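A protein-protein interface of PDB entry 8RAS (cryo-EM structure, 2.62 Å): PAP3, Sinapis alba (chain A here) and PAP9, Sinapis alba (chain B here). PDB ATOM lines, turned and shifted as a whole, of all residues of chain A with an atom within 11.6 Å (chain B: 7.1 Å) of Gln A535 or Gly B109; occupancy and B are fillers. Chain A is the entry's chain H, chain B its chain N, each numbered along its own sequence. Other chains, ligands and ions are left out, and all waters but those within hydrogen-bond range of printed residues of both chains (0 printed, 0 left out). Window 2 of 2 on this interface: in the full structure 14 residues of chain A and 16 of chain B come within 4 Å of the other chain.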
ATOM      1  N   LYS A 391      13.312  -2.289 -18.303  1.00  0.00           N
ATOM      2  CA  LYS A 391      12.580  -3.098 -19.262  1.00  0.00           C
ATOM      3  C   LYS A 391      13.100  -2.841 -20.677  1.00  0.00           C
ATOM      4  O   LYS A 391      13.481  -1.718 -21.014  1.00  0.00           O
ATOM      5  CB  LYS A 391      11.086  -2.799 -19.189  1.00  0.00           C
ATOM      6  CG  LYS A 391      10.606  -2.338 -17.821  1.00  0.00           C
ATOM      7  CD  LYS A 391      10.724  -3.446 -16.783  1.00  0.00           C
ATOM      8  CE  LYS A 391      10.747  -2.877 -15.374  1.00  0.00           C
ATOM      9  NZ  LYS A 391      11.662  -3.641 -14.481  1.00  0.00           N
ATOM     10  N   PRO A 392      13.126  -3.875 -21.526  1.00  0.00           N
ATOM     11  CA  PRO A 392      13.744  -3.713 -22.853  1.00  0.00           C
ATOM     12  C   PRO A 392      12.913  -2.914 -23.839  1.00  0.00           C
ATOM     13  O   PRO A 392      13.494  -2.306 -24.750  1.00  0.00           O
ATOM     14  CB  PRO A 392      13.932  -5.156 -23.349  1.00  0.00           C
ATOM     15  CG  PRO A 392      13.225  -6.042 -22.390  1.00  0.00           C
ATOM     16  CD  PRO A 392      12.668  -5.249 -21.261  1.00  0.00           C
ATOM     17  N   GLU A 393      11.587  -2.890 -23.705  1.00  0.00           N
ATOM     18  CA  GLU A 393      10.755  -2.176 -24.665  1.00  0.00           C
ATOM     19  C   GLU A 393      10.540  -0.712 -24.304  1.00  0.00           C
ATOM     20  O   GLU A 393       9.991   0.034 -25.123  1.00  0.00           O
ATOM     21  CB  GLU A 393       9.400  -2.878 -24.826  1.00  0.00           C
ATOM     22  CG  GLU A 393       8.447  -2.715 -23.661  1.00  0.00           C
ATOM     23  CD  GLU A 393       8.486  -3.891 -22.706  1.00  0.00           C
ATOM     24  OE1 GLU A 393       9.412  -4.721 -22.822  1.00  0.00           O
ATOM     25  OE2 GLU A 393       7.589  -3.986 -21.842  1.00  0.00           O
ATOM     26  N   GLU A 394      10.952  -0.281 -23.113  1.00  0.00           N
ATOM     27  CA  GLU A 394      10.937   1.136 -22.772  1.00  0.00           C
ATOM     28  C   GLU A 394      12.201   1.863 -23.212  1.00  0.00           C
ATOM     29  O   GLU A 394      12.219   3.099 -23.207  1.00  0.00           O
ATOM     30  CB  GLU A 394      10.748   1.332 -21.261  1.00  0.00           C
ATOM     31  CG  GLU A 394       9.308   1.224 -20.764  1.00  0.00           C
ATOM     32  CD  GLU A 394       8.657  -0.106 -21.083  1.00  0.00           C
ATOM     33  OE1 GLU A 394       7.411  -0.160 -21.147  1.00  0.00           O
ATOM     34  OE2 GLU A 394       9.388  -1.105 -21.238  1.00  0.00           O
ATOM     35  N   ALA A 526       8.171  -6.234 -33.520  1.00  0.00           N
ATOM     36  CA  ALA A 526       8.141  -7.668 -33.258  1.00  0.00           C
ATOM     37  C   ALA A 526       8.239  -7.943 -31.763  1.00  0.00           C
ATOM     38  O   ALA A 526       7.589  -8.857 -31.243  1.00  0.00           O
ATOM     39  CB  ALA A 526       9.269  -8.364 -34.017  1.00  0.00           C
ATOM     40  N   LEU A 527       9.022  -7.129 -31.052  1.00  0.00           N
ATOM     41  CA  LEU A 527       9.186  -7.298 -29.615  1.00  0.00           C
ATOM     42  C   LEU A 527       7.876  -7.064 -28.872  1.00  0.00           C
ATOM     43  O   LEU A 527       7.480  -7.879 -28.033  1.00  0.00           O
ATOM     44  CB  LEU A 527      10.274  -6.343 -29.128  1.00  0.00           C
ATOM     45  CG  LEU A 527      11.015  -6.595 -27.822  1.00  0.00           C
ATOM     46  CD1 LEU A 527      12.478  -6.394 -28.091  1.00  0.00           C
ATOM     47  CD2 LEU A 527      10.569  -5.629 -26.756  1.00  0.00           C
ATOM     48  N   LEU A 528       7.188  -5.961 -29.175  1.00  0.00           N
ATOM     49  CA  LEU A 528       5.910  -5.677 -28.525  1.00  0.00           C
ATOM     50  C   LEU A 528       4.880  -6.755 -28.833  1.00  0.00           C
ATOM     51  O   LEU A 528       4.097  -7.144 -27.955  1.00  0.00           O
ATOM     52  CB  LEU A 528       5.383  -4.300 -28.934  1.00  0.00           C
ATOM     53  CG  LEU A 528       5.867  -3.045 -28.196  1.00  0.00           C
ATOM     54  CD1 LEU A 528       5.357  -3.076 -26.763  1.00  0.00           C
ATOM     55  CD2 LEU A 528       7.375  -2.879 -28.214  1.00  0.00           C
ATOM     56  N   ARG A 529       4.857  -7.251 -30.073  1.00  0.00           N
ATOM     57  CA  ARG A 529       3.980  -8.379 -30.365  1.00  0.00           C
ATOM     58  C   ARG A 529       4.356  -9.601 -29.532  1.00  0.00           C
ATOM     59  O   ARG A 529       3.474 -10.352 -29.093  1.00  0.00           O
ATOM     60  CB  ARG A 529       4.015  -8.711 -31.857  1.00  0.00           C
ATOM     61  CG  ARG A 529       3.554  -7.571 -32.749  1.00  0.00           C
ATOM     62  CD  ARG A 529       3.209  -8.057 -34.148  1.00  0.00           C
ATOM     63  NE  ARG A 529       4.357  -8.051 -35.046  1.00  0.00           N
ATOM     64  CZ  ARG A 529       4.793  -9.113 -35.709  1.00  0.00           C
ATOM     65  NH1 ARG A 529       4.195 -10.289 -35.601  1.00  0.00           N
ATOM     66  NH2 ARG A 529       5.852  -8.993 -36.505  1.00  0.00           N
ATOM     67  N   ASP A 530       5.655  -9.805 -29.296  1.00  0.00           N
ATOM     68  CA  ASP A 530       6.097 -10.911 -28.452  1.00  0.00           C
ATOM     69  C   ASP A 530       5.597 -10.752 -27.020  1.00  0.00           C
ATOM     70  O   ASP A 530       5.133 -11.718 -26.408  1.00  0.00           O
ATOM     71  CB  ASP A 530       7.623 -11.013 -28.479  1.00  0.00           C
ATOM     72  CG  ASP A 530       8.127 -11.884 -29.609  1.00  0.00           C
ATOM     73  OD1 ASP A 530       7.767 -13.079 -29.651  1.00  0.00           O
ATOM     74  OD2 ASP A 530       8.886 -11.370 -30.455  1.00  0.00           O
ATOM     75  N   ILE A 531       5.701  -9.542 -26.461  1.00  0.00           N
ATOM     76  CA  ILE A 531       5.161  -9.311 -25.118  1.00  0.00           C
ATOM     77  C   ILE A 531       3.664  -9.579 -25.087  1.00  0.00           C
ATOM     78  O   ILE A 531       3.158 -10.234 -24.165  1.00  0.00           O
ATOM     79  CB  ILE A 531       5.487  -7.897 -24.586  1.00  0.00           C
ATOM     80  CG1 ILE A 531       6.983  -7.694 -24.338  1.00  0.00           C
ATOM     81  CG2 ILE A 531       4.666  -7.562 -23.351  1.00  0.00           C
ATOM     82  CD1 ILE A 531       7.669  -6.861 -25.336  1.00  0.00           C
ATOM     83  N   SER A 532       2.933  -9.084 -26.086  1.00  0.00           N
ATOM     84  CA  SER A 532       1.491  -9.316 -26.119  1.00  0.00           C
ATOM     85  C   SER A 532       1.181 -10.807 -26.097  1.00  0.00           C
ATOM     86  O   SER A 532       0.424 -11.286 -25.242  1.00  0.00           O
ATOM     87  CB  SER A 532       0.882  -8.658 -27.357  1.00  0.00           C
ATOM     88  OG  SER A 532       0.947  -9.524 -28.476  1.00  0.00           O
ATOM     89  N   SER A 533       1.803 -11.567 -27.003  1.00  0.00           N
ATOM     90  CA  SER A 533       1.527 -12.998 -27.088  1.00  0.00           C
ATOM     91  C   SER A 533       1.932 -13.726 -25.810  1.00  0.00           C
ATOM     92  O   SER A 533       1.187 -14.579 -25.312  1.00  0.00           O
ATOM     93  CB  SER A 533       2.247 -13.595 -28.297  1.00  0.00           C
ATOM     94  OG  SER A 533       1.944 -12.870 -29.476  1.00  0.00           O
ATOM     95  N   ARG A 534       3.104 -13.400 -25.258  1.00  0.00           N
ATOM     96  CA  ARG A 534       3.617 -14.145 -24.113  1.00  0.00           C
ATOM     97  C   ARG A 534       2.798 -13.875 -22.856  1.00  0.00           C
ATOM     98  O   ARG A 534       2.426 -14.810 -22.139  1.00  0.00           O
ATOM     99  CB  ARG A 534       5.094 -13.815 -23.892  1.00  0.00           C
ATOM    100  CG  ARG A 534       6.007 -14.404 -24.958  1.00  0.00           C
ATOM    101  CD  ARG A 534       7.445 -13.941 -24.797  1.00  0.00           C
ATOM    102  NE  ARG A 534       8.307 -14.468 -25.848  1.00  0.00           N
ATOM    103  CZ  ARG A 534       8.745 -15.718 -25.906  1.00  0.00           C
ATOM    104  NH1 ARG A 534       8.418 -16.609 -24.984  1.00  0.00           N
ATOM    105  NH2 ARG A 534       9.532 -16.085 -26.913  1.00  0.00           N
ATOM    106  N   GLN A 535       2.504 -12.604 -22.565  1.00  0.00           N
ATOM    107  CA  GLN A 535       1.621 -12.310 -21.442  1.00  0.00           C
ATOM    108  C   GLN A 535       0.196 -12.785 -21.679  1.00  0.00           C
ATOM    109  O   GLN A 535      -0.547 -12.969 -20.709  1.00  0.00           O
ATOM    110  CB  GLN A 535       1.638 -10.816 -21.125  1.00  0.00           C
ATOM    111  CG  GLN A 535       2.592 -10.441 -20.002  1.00  0.00           C
ATOM    112  CD  GLN A 535       3.855  -9.787 -20.500  1.00  0.00           C
ATOM    113  OE1 GLN A 535       4.275 -10.019 -21.629  1.00  0.00           O
ATOM    114  NE2 GLN A 535       4.459  -8.948 -19.667  1.00  0.00           N
ATOM    115  N   ALA A 536      -0.209 -12.989 -22.934  1.00  0.00           N
ATOM    116  CA  ALA A 536      -1.488 -13.645 -23.168  1.00  0.00           C
ATOM    117  C   ALA A 536      -1.413 -15.145 -22.914  1.00  0.00           C
ATOM    118  O   ALA A 536      -2.434 -15.766 -22.600  1.00  0.00           O
ATOM    119  CB  ALA A 536      -1.962 -13.377 -24.596  1.00  0.00           C
ATOM    120  N   LEU A 537      -0.226 -15.740 -23.040  1.00  0.00           N
ATOM    121  CA  LEU A 537      -0.073 -17.181 -22.907  1.00  0.00           C
ATOM    122  C   LEU A 537       0.853 -17.605 -21.773  1.00  0.00           C
ATOM    123  O   LEU A 537       1.096 -18.807 -21.613  1.00  0.00           O
ATOM    124  CB  LEU A 537       0.429 -17.778 -24.228  1.00  0.00           C
ATOM    125  CG  LEU A 537      -0.564 -17.644 -25.382  1.00  0.00           C
ATOM    126  CD1 LEU A 537       0.137 -17.785 -26.718  1.00  0.00           C
ATOM    127  CD2 LEU A 537      -1.684 -18.661 -25.248  1.00  0.00           C
ATOM    128  N   GLY A 538       1.378 -16.668 -20.987  1.00  0.00           N
ATOM    129  CA  GLY A 538       2.170 -17.019 -19.826  1.00  0.00           C
ATOM    130  C   GLY A 538       3.591 -17.450 -20.102  1.00  0.00           C
ATOM    131  O   GLY A 538       4.274 -17.898 -19.174  1.00  0.00           O
ATOM    132  N   LEU A 539       4.063 -17.337 -21.341  1.00  0.00           N
ATOM    133  CA  LEU A 539       5.432 -17.712 -21.650  1.00  0.00           C
ATOM    134  C   LEU A 539       6.412 -16.731 -21.005  1.00  0.00           C
ATOM    135  O   LEU A 539       6.078 -15.565 -20.780  1.00  0.00           O
ATOM    136  CB  LEU A 539       5.648 -17.748 -23.160  1.00  0.00           C
ATOM    137  CG  LEU A 539       5.238 -19.036 -23.874  1.00  0.00           C
ATOM    138  CD1 LEU A 539       5.104 -18.792 -25.363  1.00  0.00           C
ATOM    139  CD2 LEU A 539       6.239 -20.144 -23.601  1.00  0.00           C
ATOM    140  N   PRO A 540       7.624 -17.182 -20.688  1.00  0.00           N
ATOM    141  CA  PRO A 540       8.607 -16.279 -20.081  1.00  0.00           C
ATOM    142  C   PRO A 540       9.017 -15.166 -21.030  1.00  0.00           C
ATOM    143  O   PRO A 540       9.073 -15.341 -22.250  1.00  0.00           O
ATOM    144  CB  PRO A 540       9.790 -17.202 -19.767  1.00  0.00           C
ATOM    145  CG  PRO A 540       9.639 -18.339 -20.715  1.00  0.00           C
ATOM    146  CD  PRO A 540       8.160 -18.544 -20.852  1.00  0.00           C
ATOM    147  N   LEU A 541       9.307 -14.003 -20.448  1.00  0.00           N
ATOM    148  CA  LEU A 541       9.737 -12.840 -21.216  1.00  0.00           C
ATOM    149  C   LEU A 541      11.241 -12.870 -21.470  1.00  0.00           C
ATOM    150  O   LEU A 541      11.687 -12.834 -22.621  1.00  0.00           O
ATOM    151  CB  LEU A 541       9.339 -11.554 -20.486  1.00  0.00           C
ATOM    152  CG  LEU A 541       7.847 -11.224 -20.487  1.00  0.00           C
ATOM    153  CD1 LEU A 541       7.572 -10.023 -19.600  1.00  0.00           C
ATOM    154  CD2 LEU A 541       7.357 -10.980 -21.904  1.00  0.00           C
ATOM    155  N   GLU A 542      12.031 -12.933 -20.404  1.00  0.00           N
ATOM    156  CA  GLU A 542      13.473 -13.065 -20.517  1.00  0.00           C
ATOM    157  C   GLU A 542      13.876 -14.530 -20.381  1.00  0.00           C
ATOM    158  O   GLU A 542      13.077 -15.391 -20.002  1.00  0.00           O
ATOM    159  CB  GLU A 542      14.172 -12.206 -19.463  1.00  0.00           C
ATOM    160  CG  GLU A 542      13.492 -10.871 -19.210  1.00  0.00           C
ATOM    161  CD  GLU A 542      14.467  -9.711 -19.184  1.00  0.00           C
ATOM    162  OE1 GLU A 542      14.136  -8.669 -18.580  1.00  0.00           O
ATOM    163  OE2 GLU A 542      15.564  -9.840 -19.767  1.00  0.00           O
ATOM    164  N   SER B 105      -6.346  -0.868 -19.513  1.00  0.00           N
ATOM    165  CA  SER B 105      -6.240  -2.172 -18.876  1.00  0.00           C
ATOM    166  C   SER B 105      -5.079  -3.000 -19.410  1.00  0.00           C
ATOM    167  O   SER B 105      -4.639  -3.931 -18.726  1.00  0.00           O
ATOM    168  CB  SER B 105      -7.552  -2.938 -19.044  1.00  0.00           C
ATOM    169  OG  SER B 105      -7.934  -3.011 -20.406  1.00  0.00           O
ATOM    170  N   TYR B 106      -4.578  -2.694 -20.610  1.00  0.00           N
ATOM    171  CA  TYR B 106      -3.380  -3.377 -21.092  1.00  0.00           C
ATOM    172  C   TYR B 106      -2.177  -3.047 -20.218  1.00  0.00           C
ATOM    173  O   TYR B 106      -1.354  -3.923 -19.925  1.00  0.00           O
ATOM    174  CB  TYR B 106      -3.106  -3.007 -22.549  1.00  0.00           C
ATOM    175  CG  TYR B 106      -1.875  -3.674 -23.119  1.00  0.00           C
ATOM    176  CD1 TYR B 106      -1.872  -5.031 -23.415  1.00  0.00           C
ATOM    177  CD2 TYR B 106      -0.716  -2.950 -23.360  1.00  0.00           C
ATOM    178  CE1 TYR B 106      -0.749  -5.647 -23.935  1.00  0.00           C
ATOM    179  CE2 TYR B 106       0.411  -3.557 -23.881  1.00  0.00           C
ATOM    180  CZ  TYR B 106       0.388  -4.906 -24.166  1.00  0.00           C
ATOM    181  OH  TYR B 106       1.509  -5.514 -24.683  1.00  0.00           O
ATOM    182  N   ASN B 107      -2.053  -1.783 -19.806  1.00  0.00           N
ATOM    183  CA  ASN B 107      -1.056  -1.346 -18.826  1.00  0.00           C
ATOM    184  C   ASN B 107       0.374  -1.596 -19.302  1.00  0.00           C
ATOM    185  O   ASN B 107       1.281  -1.779 -18.490  1.00  0.00           O
ATOM    186  CB  ASN B 107      -1.291  -2.015 -17.468  1.00  0.00           C
ATOM    187  CG  ASN B 107      -0.874  -1.137 -16.303  1.00  0.00           C
ATOM    188  OD1 ASN B 107       0.123  -0.419 -16.373  1.00  0.00           O
ATOM    189  ND2 ASN B 107      -1.641  -1.193 -15.219  1.00  0.00           N
ATOM    190  N   ARG B 108       0.589  -1.585 -20.618  1.00  0.00           N
ATOM    191  CA  ARG B 108       1.914  -1.800 -21.205  1.00  0.00           C
ATOM    192  C   ARG B 108       2.489  -3.165 -20.824  1.00  0.00           C
ATOM    193  O   ARG B 108       3.678  -3.296 -20.528  1.00  0.00           O
ATOM    194  CB  ARG B 108       2.883  -0.680 -20.818  1.00  0.00           C
ATOM    195  CG  ARG B 108       3.200   0.295 -21.937  1.00  0.00           C
ATOM    196  CD  ARG B 108       4.122   1.397 -21.446  1.00  0.00           C
ATOM    197  NE  ARG B 108       3.620   2.025 -20.230  1.00  0.00           N
ATOM    198  CZ  ARG B 108       3.999   3.217 -19.790  1.00  0.00           C
ATOM    199  NH1 ARG B 108       4.891   3.943 -20.444  1.00  0.00           N
ATOM    200  NH2 ARG B 108       3.472   3.692 -18.665  1.00  0.00           N
ATOM    201  N   GLY B 109       1.640  -4.190 -20.831  1.00  0.00           N
ATOM    202  CA  GLY B 109       2.109  -5.555 -20.682  1.00  0.00           C
ATOM    203  C   GLY B 109       1.586  -6.326 -19.486  1.00  0.00           C
ATOM    204  O   GLY B 109       1.218  -7.495 -19.626  1.00  0.00           O
ATOM    205  N   ASN B 110       1.539  -5.702 -18.309  1.00  0.00           N
ATOM    206  CA  ASN B 110       0.984  -6.360 -17.124  1.00  0.00           C
ATOM    207  C   ASN B 110      -0.505  -6.042 -17.088  1.00  0.00           C
ATOM    208  O   ASN B 110      -0.942  -5.054 -16.498  1.00  0.00           O
ATOM    209  CB  ASN B 110       1.702  -5.920 -15.853  1.00  0.00           C
ATOM    210  CG  ASN B 110       1.986  -4.436 -15.825  1.00  0.00           C
ATOM    211  OD1 ASN B 110       1.659  -3.716 -16.762  1.00  0.00           O
ATOM    212  ND2 ASN B 110       2.597  -3.970 -14.742  1.00  0.00           N
ATOM    213  N   MET B 111      -1.289  -6.902 -17.734  1.00  0.00           N
ATOM    214  CA  MET B 111      -2.704  -6.630 -17.943  1.00  0.00           C
ATOM    215  C   MET B 111      -3.462  -6.588 -16.623  1.00  0.00           C
ATOM    216  O   MET B 111      -3.275  -7.437 -15.747  1.00  0.00           O
ATOM    217  CB  MET B 111      -3.307  -7.692 -18.864  1.00  0.00           C
ATOM    218  CG  MET B 111      -2.645  -7.769 -20.231  1.00  0.00           C
ATOM    219  SD  MET B 111      -2.514  -9.454 -20.861  1.00  0.00           S
ATOM    220  CE  MET B 111      -3.993 -10.197 -20.175  1.00  0.00           C
ATOM    221  N   LEU B 112      -4.326  -5.585 -16.488  1.00  0.00           N
ATOM    222  CA  LEU B 112      -5.195  -5.478 -15.332  1.00  0.00           C
ATOM    223  C   LEU B 112      -6.277  -6.555 -15.394  1.00  0.00           C
ATOM    224  O   LEU B 112      -6.559  -7.101 -16.463  1.00  0.00           O
ATOM    225  CB  LEU B 112      -5.825  -4.088 -15.276  1.00  0.00           C
ATOM    226  CG  LEU B 112      -4.931  -2.970 -14.735  1.00  0.00           C
ATOM    227  CD1 LEU B 112      -5.618  -1.620 -14.867  1.00  0.00           C
ATOM    228  CD2 LEU B 112      -4.546  -3.243 -13.288  1.00  0.00           C
ATOM    229  N   PRO B 206      -3.442 -14.290 -29.486  1.00  0.00           N
ATOM    230  CA  PRO B 206      -4.125 -15.279 -28.652  1.00  0.00           C
ATOM    231  C   PRO B 206      -5.058 -14.648 -27.631  1.00  0.00           C
ATOM    232  O   PRO B 206      -4.830 -13.547 -27.126  1.00  0.00           O
ATOM    233  CB  PRO B 206      -2.959 -15.995 -27.958  1.00  0.00           C
ATOM    234  CG  PRO B 206      -1.899 -14.941 -27.842  1.00  0.00           C
ATOM    235  CD  PRO B 206      -2.123 -13.925 -28.941  1.00  0.00           C
ATOM    236  N   ASN B 207      -6.131 -15.382 -27.336  1.00  0.00           N
ATOM    237  CA  ASN B 207      -7.119 -15.018 -26.315  1.00  0.00           C
ATOM    238  C   ASN B 207      -7.767 -13.697 -26.714  1.00  0.00           C
ATOM    239  O   ASN B 207      -8.352 -13.627 -27.807  1.00  0.00           O
ATOM    240  CB  ASN B 207      -6.443 -15.043 -24.942  1.00  0.00           C
ATOM    241  CG  ASN B 207      -5.606 -16.287 -24.728  1.00  0.00           C
ATOM    242  OD1 ASN B 207      -5.927 -17.359 -25.240  1.00  0.00           O
ATOM    243  ND2 ASN B 207      -4.526 -16.150 -23.969  1.00  0.00           N
ATOM    244  N   VAL B 209      -6.279 -10.619 -27.080  1.00  0.00           N
ATOM    245  CA  VAL B 209      -5.358  -9.596 -27.555  1.00  0.00           C
ATOM    246  C   VAL B 209      -5.814  -9.076 -28.911  1.00  0.00           C
ATOM    247  O   VAL B 209      -6.208  -9.848 -29.796  1.00  0.00           O
ATOM    248  CB  VAL B 209      -3.926 -10.153 -27.618  1.00  0.00           C
ATOM    249  CG1 VAL B 209      -2.973  -9.125 -28.205  1.00  0.00           C
ATOM    250  CG2 VAL B 209      -3.468 -10.568 -26.234  1.00  0.00           C
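ND2 of Asn B207 lies within hydrogen-bond range of O of Ala A536.
Among the printed residues, pairs that only touch across the chains: Gln A535 with Gly B109 (3.3 Å), Ala A536 with Val B209 (3.6 Å), Ala A536 with Pro B206 (3.6 Å), Glu A394 with Arg B108 (3.7 Å), Leu A537 with Pro B206 (3.7 Å), Ser A532 with Val B209 (3.9 Å) and Ile A531 with Tyr B106 (3.99 Å).
Gln A535 touches one residue of chain B.
Of chain A, only Gln A535 (3.3 Å) comes within 4 Å of Gly B109.
No residue of chain A comes within 4 Å of Asn B107.
No residue of chain A comes within 4 Å of Met B111.
Printed residues of chain A within 4 Å of Tyr B106: Ile A531 (3.99 Å).
Printed residues of chain A within 4 Å of Val B209: Ser A532 and Ala A536.
Of the printed residues of chain B, Ser A532 touches Val B209 (3.9 Å).
Printed residues of chain B within 4 Å of Ile A531: Tyr B106.
Of the printed residues of chain B, Glu A394 touches Arg B108 (3.7 Å).
The nearest residue of chain B that does not touch Gln A535 is Met B111 (4.03 Å).
The backbone carbonyl oxygen (O) of Arg A529 is in hydrogen-bond range of the side-chain hydroxyl (OG) of Ser A532 (2.7 Å).
O of Ile A531 sits close to OE1 of Gln A535, at 2.8 Å.
Of the 21 printed residues of chain A, 6 touch a printed residue of chain B.
Hydrophobic or aromatic side chains of chain A that line the printed part of chain B: Ile A531, Ala A536 and Leu A537.
Of the 11 printed residues of chain B, 6 touch a printed residue of chain A.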
